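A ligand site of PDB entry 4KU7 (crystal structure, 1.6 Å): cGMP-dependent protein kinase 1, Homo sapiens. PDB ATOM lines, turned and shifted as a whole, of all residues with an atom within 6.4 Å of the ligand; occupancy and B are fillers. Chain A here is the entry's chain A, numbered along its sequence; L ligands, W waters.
The backbone NH (N) of Thr 101 lies within hydrogen-bond range of an oxygen (O2) of the ligand, 2.7 Å away.
The backbone NH (N) of Ala 93 sits at hydrogen-bond distance from an oxygen (O1) of the ligand (2.9 Å).
The backbone NH (N) of Gly 90 sits at hydrogen-bond distance from an oxygen (O6) of the ligand (2.8 Å).
The backbone NH (N) of Lys 92 sits at hydrogen-bond distance from an oxygen (O1) of the ligand (3.3 Å).
OH of Tyr 135 lies within hydrogen-bond range of O6 of the ligand, 3.1 Å away.
OG1 of Thr 101 sits at hydrogen-bond distance from O2 of the ligand (2.6 Å).
NH1 of Arg 100 lies within salt-bridge range of O1 of the ligand (2.9 Å).
The side-chain carboxylate (OE1) of Glu 91 is in hydrogen-bond range of an oxygen (O6) of the ligand (2.5 Å).
A nitrogen (N2) of the ligand sits at hydrogen-bond distance from the guanidinium group (NE) of Arg 81 (2.7 Å).
Water W1 lies within hydrogen-bond range of O of Trp 88 (2.7 Å), OH of Tyr 135 (2.9 Å) and O6 of the ligand (3.5 Å).
N of Leu 80 is in hydrogen-bond range of O of Val 67 (2.8 Å).
O of Ile 48 sits at hydrogen-bond distance from N of Val 104, at 3.0 Å.
The guanidinium group of Arg 100 sits at hydrogen-bond distance from the backbone carbonyl oxygen of Gly 90 (2.9 Å).
The backbone carbonyl oxygen (O) of Thr 101 is in hydrogen-bond range of the guanidinium group (NH1) of Arg 69 (2.6 Å).
The guanidinium group (NH2) of Arg 100 is in hydrogen-bond range of the backbone carbonyl oxygen (O) of Thr 56 (2.9 Å).
OE2 of Glu 91 is in hydrogen-bond range of OH of Tyr 135 (2.6 Å).
The backbone NH (N) of Val 67 lies within hydrogen-bond range of the backbone carbonyl oxygen (O) of Arg 81, at 2.8 Å.
NZ of Lys 92 is in salt-bridge range of OE2 of Glu 91 (2.7 Å).
Merely in contact with the ligand: Ile 48 (3.7 Å), Val 67 (3.7 Å), Leu 80 (3.4 Å), Phe 89 (3.2 Å), Ala 102 (3.4 Å) and Val 104 (3.7 Å).
Hydrophobic or aromatic side chains within 4 Å of the ligand: Ile 48, Val 67, Leu 80, Phe 89, Ala 93, Ala 102, Val 104 and Tyr 135.
Of the 22 residues printed, 14 come within 4 Å of the ligand.
The nearest printed residue that does not touch the ligand is Leu 83 (4.3 Å).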
ATOM      1  N   ILE A  48      21.159  18.018 -20.788  1.00  0.00           N
ATOM      2  CA  ILE A  48      21.883  18.452 -19.591  1.00  0.00           C
ATOM      3  C   ILE A  48      20.853  18.802 -18.543  1.00  0.00           C
ATOM      4  O   ILE A  48      19.822  19.392 -18.863  1.00  0.00           O
ATOM      5  CB  ILE A  48      22.718  19.717 -19.862  1.00  0.00           C
ATOM      6  CG1 ILE A  48      23.955  19.378 -20.697  1.00  0.00           C
ATOM      7  CG2 ILE A  48      23.146  20.383 -18.549  1.00  0.00           C
ATOM      8  CD1 ILE A  48      24.744  20.626 -21.153  1.00  0.00           C
ATOM      9  N   THR A  56      31.615  17.892 -20.406  1.00  0.00           N
ATOM     10  CA  THR A  56      31.459  17.823 -21.866  1.00  0.00           C
ATOM     11  C   THR A  56      30.862  19.089 -22.454  1.00  0.00           C
ATOM     12  O   THR A  56      30.033  19.766 -21.830  1.00  0.00           O
ATOM     13  CB  THR A  56      30.575  16.642 -22.302  1.00  0.00           C
ATOM     14  OG1 THR A  56      29.452  16.544 -21.418  1.00  0.00           O
ATOM     15  CG2 THR A  56      31.364  15.325 -22.247  1.00  0.00           C
ATOM     16  N   PHE A  57      31.295  19.390 -23.670  1.00  0.00           N
ATOM     17  CA  PHE A  57      30.867  20.549 -24.451  1.00  0.00           C
ATOM     18  C   PHE A  57      30.109  20.027 -25.662  1.00  0.00           C
ATOM     19  O   PHE A  57      30.484  18.995 -26.208  1.00  0.00           O
ATOM     20  CB  PHE A  57      32.132  21.301 -24.898  1.00  0.00           C
ATOM     21  CG  PHE A  57      31.872  22.534 -25.729  1.00  0.00           C
ATOM     22  CD1 PHE A  57      31.346  23.691 -25.160  1.00  0.00           C
ATOM     23  CD2 PHE A  57      32.217  22.547 -27.075  1.00  0.00           C
ATOM     24  CE1 PHE A  57      31.125  24.824 -25.930  1.00  0.00           C
ATOM     25  CE2 PHE A  57      32.011  23.690 -27.857  1.00  0.00           C
ATOM     26  CZ  PHE A  57      31.465  24.829 -27.296  1.00  0.00           C
ATOM     27  N   VAL A  67      16.636  25.781 -23.622  1.00  0.00           N
ATOM     28  CA  VAL A  67      17.439  25.994 -22.420  1.00  0.00           C
ATOM     29  C   VAL A  67      16.530  26.595 -21.358  1.00  0.00           C
ATOM     30  O   VAL A  67      15.814  27.552 -21.626  1.00  0.00           O
ATOM     31  CB  VAL A  67      18.598  26.969 -22.671  1.00  0.00           C
ATOM     32  CG1 VAL A  67      19.491  27.065 -21.440  1.00  0.00           C
ATOM     33  CG2 VAL A  67      19.409  26.499 -23.870  1.00  0.00           C
ATOM     34  N   ARG A  69      16.167  27.356 -16.758  1.00  0.00           N
ATOM     35  CA  ARG A  69      16.945  27.462 -15.525  1.00  0.00           C
ATOM     36  C   ARG A  69      16.105  27.824 -14.303  1.00  0.00           C
ATOM     37  O   ARG A  69      15.127  28.563 -14.413  1.00  0.00           O
ATOM     38  CB  ARG A  69      18.082  28.482 -15.682  1.00  0.00           C
ATOM     39  CG  ARG A  69      18.766  28.872 -14.367  1.00  0.00           C
ATOM     40  CD  ARG A  69      20.033  29.682 -14.593  1.00  0.00           C
ATOM     41  NE  ARG A  69      20.464  30.341 -13.366  1.00  0.00           N
ATOM     42  CZ  ARG A  69      21.305  29.817 -12.482  1.00  0.00           C
ATOM     43  NH1 ARG A  69      21.820  28.606 -12.696  1.00  0.00           N
ATOM     44  NH2 ARG A  69      21.641  30.485 -11.388  1.00  0.00           N
ATOM     45  N   LEU A  80      14.825  30.070 -21.082  1.00  0.00           N
ATOM     46  CA  LEU A  80      15.844  31.071 -21.376  1.00  0.00           C
ATOM     47  C   LEU A  80      15.954  31.351 -22.871  1.00  0.00           C
ATOM     48  O   LEU A  80      15.866  32.498 -23.296  1.00  0.00           O
ATOM     49  CB  LEU A  80      17.204  30.656 -20.806  1.00  0.00           C
ATOM     50  CG  LEU A  80      17.256  30.498 -19.291  1.00  0.00           C
ATOM     51  CD1 LEU A  80      18.676  30.198 -18.850  1.00  0.00           C
ATOM     52  CD2 LEU A  80      16.730  31.750 -18.603  1.00  0.00           C
ATOM     53  N   ARG A  81      16.112  30.301 -23.658  1.00  0.00           N
ATOM     54  CA  ARG A  81      16.294  30.466 -25.087  1.00  0.00           C
ATOM     55  C   ARG A  81      16.300  29.136 -25.828  1.00  0.00           C
ATOM     56  O   ARG A  81      16.391  28.069 -25.211  1.00  0.00           O
ATOM     57  CB  ARG A  81      17.623  31.189 -25.353  1.00  0.00           C
ATOM     58  CG  ARG A  81      18.841  30.301 -25.224  1.00  0.00           C
ATOM     59  CD  ARG A  81      20.141  31.089 -25.335  1.00  0.00           C
ATOM     60  NE  ARG A  81      20.440  31.835 -24.118  1.00  0.00           N
ATOM     61  CZ  ARG A  81      20.220  33.133 -23.944  1.00  0.00           C
ATOM     62  NH1 ARG A  81      19.717  33.870 -24.941  1.00  0.00           N
ATOM     63  NH2 ARG A  81      20.528  33.707 -22.793  1.00  0.00           N
ATOM     64  N   LEU A  83      18.351  27.031 -28.959  1.00  0.00           N
ATOM     65  CA  LEU A  83      19.574  26.992 -29.744  1.00  0.00           C
ATOM     66  C   LEU A  83      19.405  26.029 -30.919  1.00  0.00           C
ATOM     67  O   LEU A  83      18.648  25.064 -30.829  1.00  0.00           O
ATOM     68  CB  LEU A  83      20.760  26.567 -28.875  1.00  0.00           C
ATOM     69  CG  LEU A  83      21.060  27.472 -27.682  1.00  0.00           C
ATOM     70  CD1 LEU A  83      22.118  26.851 -26.794  1.00  0.00           C
ATOM     71  CD2 LEU A  83      21.500  28.853 -28.154  1.00  0.00           C
ATOM     72  N   TRP A  88      26.208  26.206 -29.768  1.00  0.00           N
ATOM     73  CA  TRP A  88      26.886  25.320 -28.843  1.00  0.00           C
ATOM     74  C   TRP A  88      26.495  25.644 -27.406  1.00  0.00           C
ATOM     75  O   TRP A  88      25.933  26.714 -27.128  1.00  0.00           O
ATOM     76  CB  TRP A  88      28.397  25.402 -29.027  1.00  0.00           C
ATOM     77  CG  TRP A  88      28.903  26.812 -29.197  1.00  0.00           C
ATOM     78  CD1 TRP A  88      29.172  27.445 -30.377  1.00  0.00           C
ATOM     79  CD2 TRP A  88      29.219  27.735 -28.150  1.00  0.00           C
ATOM     80  NE1 TRP A  88      29.618  28.724 -30.124  1.00  0.00           N
ATOM     81  CE2 TRP A  88      29.664  28.921 -28.766  1.00  0.00           C
ATOM     82  CE3 TRP A  88      29.178  27.681 -26.746  1.00  0.00           C
ATOM     83  CZ2 TRP A  88      30.059  30.044 -28.032  1.00  0.00           C
ATOM     84  CZ3 TRP A  88      29.555  28.807 -26.025  1.00  0.00           C
ATOM     85  CH2 TRP A  88      29.994  29.970 -26.670  1.00  0.00           C
ATOM     86  N   PHE A  89      26.796  24.725 -26.491  1.00  0.00           N
ATOM     87  CA  PHE A  89      26.407  24.883 -25.092  1.00  0.00           C
ATOM     88  C   PHE A  89      27.207  23.908 -24.247  1.00  0.00           C
ATOM     89  O   PHE A  89      27.850  22.994 -24.772  1.00  0.00           O
ATOM     90  CB  PHE A  89      24.897  24.663 -24.912  1.00  0.00           C
ATOM     91  CG  PHE A  89      24.401  23.278 -25.335  1.00  0.00           C
ATOM     92  CD1 PHE A  89      23.929  23.052 -26.621  1.00  0.00           C
ATOM     93  CD2 PHE A  89      24.394  22.233 -24.425  1.00  0.00           C
ATOM     94  CE1 PHE A  89      23.466  21.783 -26.998  1.00  0.00           C
ATOM     95  CE2 PHE A  89      23.942  20.966 -24.810  1.00  0.00           C
ATOM     96  CZ  PHE A  89      23.479  20.749 -26.092  1.00  0.00           C
ATOM     97  N   GLY A  90      27.176  24.109 -22.936  1.00  0.00           N
ATOM     98  CA  GLY A  90      27.858  23.231 -21.990  1.00  0.00           C
ATOM     99  C   GLY A  90      29.213  23.756 -21.555  1.00  0.00           C
ATOM    100  O   GLY A  90      29.953  23.064 -20.869  1.00  0.00           O
ATOM    101  N   GLU A  91      29.552  24.976 -21.936  1.00  0.00           N
ATOM    102  CA  GLU A  91      30.867  25.500 -21.594  1.00  0.00           C
ATOM    103  C   GLU A  91      30.989  25.908 -20.125  1.00  0.00           C
ATOM    104  O   GLU A  91      32.089  25.949 -19.593  1.00  0.00           O
ATOM    105  CB  GLU A  91      31.269  26.684 -22.485  1.00  0.00           C
ATOM    106  CG  GLU A  91      30.727  28.055 -22.021  1.00  0.00           C
ATOM    107  CD  GLU A  91      29.259  28.272 -22.382  1.00  0.00           C
ATOM    108  OE1 GLU A  91      28.617  27.370 -22.947  1.00  0.00           O
ATOM    109  OE2 GLU A  91      28.748  29.376 -22.082  1.00  0.00           O
ATOM    110  N   LYS A  92      29.872  26.254 -19.479  1.00  0.00           N
ATOM    111  CA  LYS A  92      30.006  26.803 -18.135  1.00  0.00           C
ATOM    112  C   LYS A  92      30.577  25.784 -17.167  1.00  0.00           C
ATOM    113  O   LYS A  92      31.377  26.142 -16.324  1.00  0.00           O
ATOM    114  CB  LYS A  92      28.709  27.434 -17.617  1.00  0.00           C
ATOM    115  CG  LYS A  92      28.343  28.737 -18.339  1.00  0.00           C
ATOM    116  CD  LYS A  92      29.401  29.819 -18.126  1.00  0.00           C
ATOM    117  CE  LYS A  92      29.154  31.048 -19.026  1.00  0.00           C
ATOM    118  NZ  LYS A  92      29.983  31.031 -20.279  1.00  0.00           N
ATOM    119  N   ALA A  93      30.186  24.517 -17.290  1.00  0.00           N
ATOM    120  CA  ALA A  93      30.736  23.493 -16.404  1.00  0.00           C
ATOM    121  C   ALA A  93      32.215  23.221 -16.697  1.00  0.00           C
ATOM    122  O   ALA A  93      32.886  22.514 -15.938  1.00  0.00           O
ATOM    123  CB  ALA A  93      29.934  22.185 -16.512  1.00  0.00           C
ATOM    124  N   LEU A  94      32.709  23.767 -17.797  1.00  0.00           N
ATOM    125  CA  LEU A  94      34.110  23.586 -18.160  1.00  0.00           C
ATOM    126  C   LEU A  94      34.915  24.837 -17.840  1.00  0.00           C
ATOM    127  O   LEU A  94      36.092  24.917 -18.176  1.00  0.00           O
ATOM    128  CB  LEU A  94      34.235  23.239 -19.646  1.00  0.00           C
ATOM    129  CG  LEU A  94      33.497  21.960 -20.055  1.00  0.00           C
ATOM    130  CD1 LEU A  94      33.424  21.816 -21.560  1.00  0.00           C
ATOM    131  CD2 LEU A  94      34.146  20.749 -19.426  1.00  0.00           C
ATOM    132  N   VAL A  99      29.863  22.592 -12.310  1.00  0.00           N
ATOM    133  CA  VAL A  99      28.411  22.406 -12.174  1.00  0.00           C
ATOM    134  C   VAL A  99      27.661  22.944 -13.388  1.00  0.00           C
ATOM    135  O   VAL A  99      28.006  23.992 -13.941  1.00  0.00           O
ATOM    136  CB  VAL A  99      27.873  23.031 -10.877  1.00  0.00           C
ATOM    137  CG1 VAL A  99      28.191  24.522 -10.824  1.00  0.00           C
ATOM    138  CG2 VAL A  99      26.375  22.785 -10.738  1.00  0.00           C
ATOM    139  N   ARG A 100      26.631  22.209 -13.816  1.00  0.00           N
ATOM    140  CA  ARG A 100      25.747  22.673 -14.868  1.00  0.00           C
ATOM    141  C   ARG A 100      24.812  23.754 -14.355  1.00  0.00           C
ATOM    142  O   ARG A 100      24.230  23.630 -13.283  1.00  0.00           O
ATOM    143  CB  ARG A 100      24.953  21.498 -15.450  1.00  0.00           C
ATOM    144  CG  ARG A 100      25.815  20.408 -16.082  1.00  0.00           C
ATOM    145  CD  ARG A 100      26.529  20.930 -17.302  1.00  0.00           C
ATOM    146  NE  ARG A 100      27.053  19.802 -18.067  1.00  0.00           N
ATOM    147  CZ  ARG A 100      27.886  19.908 -19.086  1.00  0.00           C
ATOM    148  NH1 ARG A 100      28.285  21.099 -19.516  1.00  0.00           N
ATOM    149  NH2 ARG A 100      28.319  18.803 -19.697  1.00  0.00           N
ATOM    150  N   THR A 101      24.684  24.842 -15.119  1.00  0.00           N
ATOM    151  CA  THR A 101      23.973  26.009 -14.623  1.00  0.00           C
ATOM    152  C   THR A 101      22.570  26.161 -15.199  1.00  0.00           C
ATOM    153  O   THR A 101      21.833  27.084 -14.830  1.00  0.00           O
ATOM    154  CB  THR A 101      24.761  27.300 -14.915  1.00  0.00           C
ATOM    155  OG1 THR A 101      24.853  27.496 -16.325  1.00  0.00           O
ATOM    156  CG2 THR A 101      26.171  27.170 -14.359  1.00  0.00           C
ATOM    157  N   ALA A 102      22.199  25.262 -16.103  1.00  0.00           N
ATOM    158  CA  ALA A 102      20.891  25.312 -16.740  1.00  0.00           C
ATOM    159  C   ALA A 102      20.546  23.954 -17.327  1.00  0.00           C
ATOM    160  O   ALA A 102      21.416  23.112 -17.493  1.00  0.00           O
ATOM    161  CB  ALA A 102      20.875  26.375 -17.841  1.00  0.00           C
ATOM    162  N   ASN A 103      19.256  23.741 -17.610  1.00  0.00           N
ATOM    163  CA  ASN A 103      18.835  22.547 -18.340  1.00  0.00           C
ATOM    164  C   ASN A 103      18.888  22.793 -19.841  1.00  0.00           C
ATOM    165  O   ASN A 103      18.609  23.897 -20.301  1.00  0.00           O
ATOM    166  CB  ASN A 103      17.408  22.150 -17.960  1.00  0.00           C
ATOM    167  CG  ASN A 103      17.214  21.982 -16.474  1.00  0.00           C
ATOM    168  OD1 ASN A 103      17.731  21.046 -15.870  1.00  0.00           O
ATOM    169  ND2 ASN A 103      16.421  22.870 -15.881  1.00  0.00           N
ATOM    170  N   VAL A 104      19.269  21.770 -20.587  1.00  0.00           N
ATOM    171  CA  VAL A 104      19.180  21.803 -22.046  1.00  0.00           C
ATOM    172  C   VAL A 104      18.382  20.583 -22.497  1.00  0.00           C
ATOM    173  O   VAL A 104      18.715  19.454 -22.154  1.00  0.00           O
ATOM    174  CB  VAL A 104      20.573  21.838 -22.702  1.00  0.00           C
ATOM    175  CG1 VAL A 104      20.433  21.939 -24.223  1.00  0.00           C
ATOM    176  CG2 VAL A 104      21.396  22.991 -22.161  1.00  0.00           C
ATOM    177  N   TYR A 135      25.519  35.632 -21.004  1.00  0.00           N
ATOM    178  CA  TYR A 135      24.096  35.425 -21.236  1.00  0.00           C
ATOM    179  C   TYR A 135      23.243  36.560 -20.676  1.00  0.00           C
ATOM    180  O   TYR A 135      23.774  37.540 -20.169  1.00  0.00           O
ATOM    181  CB  TYR A 135      23.669  34.083 -20.644  1.00  0.00           C
ATOM    182  CG  TYR A 135      24.384  32.932 -21.280  1.00  0.00           C
ATOM    183  CD1 TYR A 135      25.463  32.316 -20.662  1.00  0.00           C
ATOM    184  CD2 TYR A 135      24.007  32.488 -22.537  1.00  0.00           C
ATOM    185  CE1 TYR A 135      26.127  31.262 -21.277  1.00  0.00           C
ATOM    186  CE2 TYR A 135      24.647  31.436 -23.149  1.00  0.00           C
ATOM    187  CZ  TYR A 135      25.711  30.831 -22.523  1.00  0.00           C
ATOM    188  OH  TYR A 135      26.363  29.781 -23.142  1.00  0.00           O
HETATM  189  P1  LIG L   1      26.451  24.609 -18.723  1.00  0.00           P
HETATM  190  O1  LIG L   1      27.712  23.853 -18.629  1.00  0.00           O
HETATM  191  O2  LIG L   1      25.946  25.400 -17.400  1.00  0.00           O
HETATM  192  O3  LIG L   1      25.320  23.663 -19.161  1.00  0.00           O
HETATM  193  C1  LIG L   1      23.987  24.381 -19.407  1.00  0.00           C
HETATM  194  C2  LIG L   1      24.209  25.229 -20.600  1.00  0.00           C
HETATM  195  O4  LIG L   1      23.145  26.036 -21.136  1.00  0.00           O
HETATM  196  C3  LIG L   1      25.261  26.273 -20.269  1.00  0.00           C
HETATM  197  O5  LIG L   1      26.566  25.701 -19.953  1.00  0.00           O
HETATM  198  C4  LIG L   1      25.291  27.136 -21.530  1.00  0.00           C
HETATM  199  O6  LIG L   1      26.227  26.723 -22.481  1.00  0.00           O
HETATM  200  C5  LIG L   1      23.821  26.999 -21.994  1.00  0.00           C
HETATM  201  N1  LIG L   1      23.079  28.261 -21.939  1.00  0.00           N
HETATM  202  C6  LIG L   1      22.329  28.842 -23.038  1.00  0.00           C
HETATM  203  N2  LIG L   1      21.709  30.050 -22.511  1.00  0.00           N
HETATM  204  C7  LIG L   1      22.061  30.170 -21.092  1.00  0.00           C
HETATM  205  C8  LIG L   1      21.730  31.211 -20.055  1.00  0.00           C
HETATM  206  O7  LIG L   1      20.948  32.305 -20.409  1.00  0.00           O
HETATM  207  N3  LIG L   1      22.210  31.084 -18.758  1.00  0.00           N
HETATM  208  C9  LIG L   1      23.026  29.968 -18.412  1.00  0.00           C
HETATM  209  N4  LIG L   1      23.506  29.834 -17.053  1.00  0.00           N
HETATM  210  N5  LIG L   1      23.366  28.937 -19.444  1.00  0.00           N
HETATM  211  C10 LIG L   1      22.885  29.071 -20.729  1.00  0.00           C
HETATM  212  O   HOH W   1      24.982  28.434 -25.244  1.00  0.00           O
HETATM  213  O   HOH W   2      21.739  32.766 -16.450  1.00  0.00           O
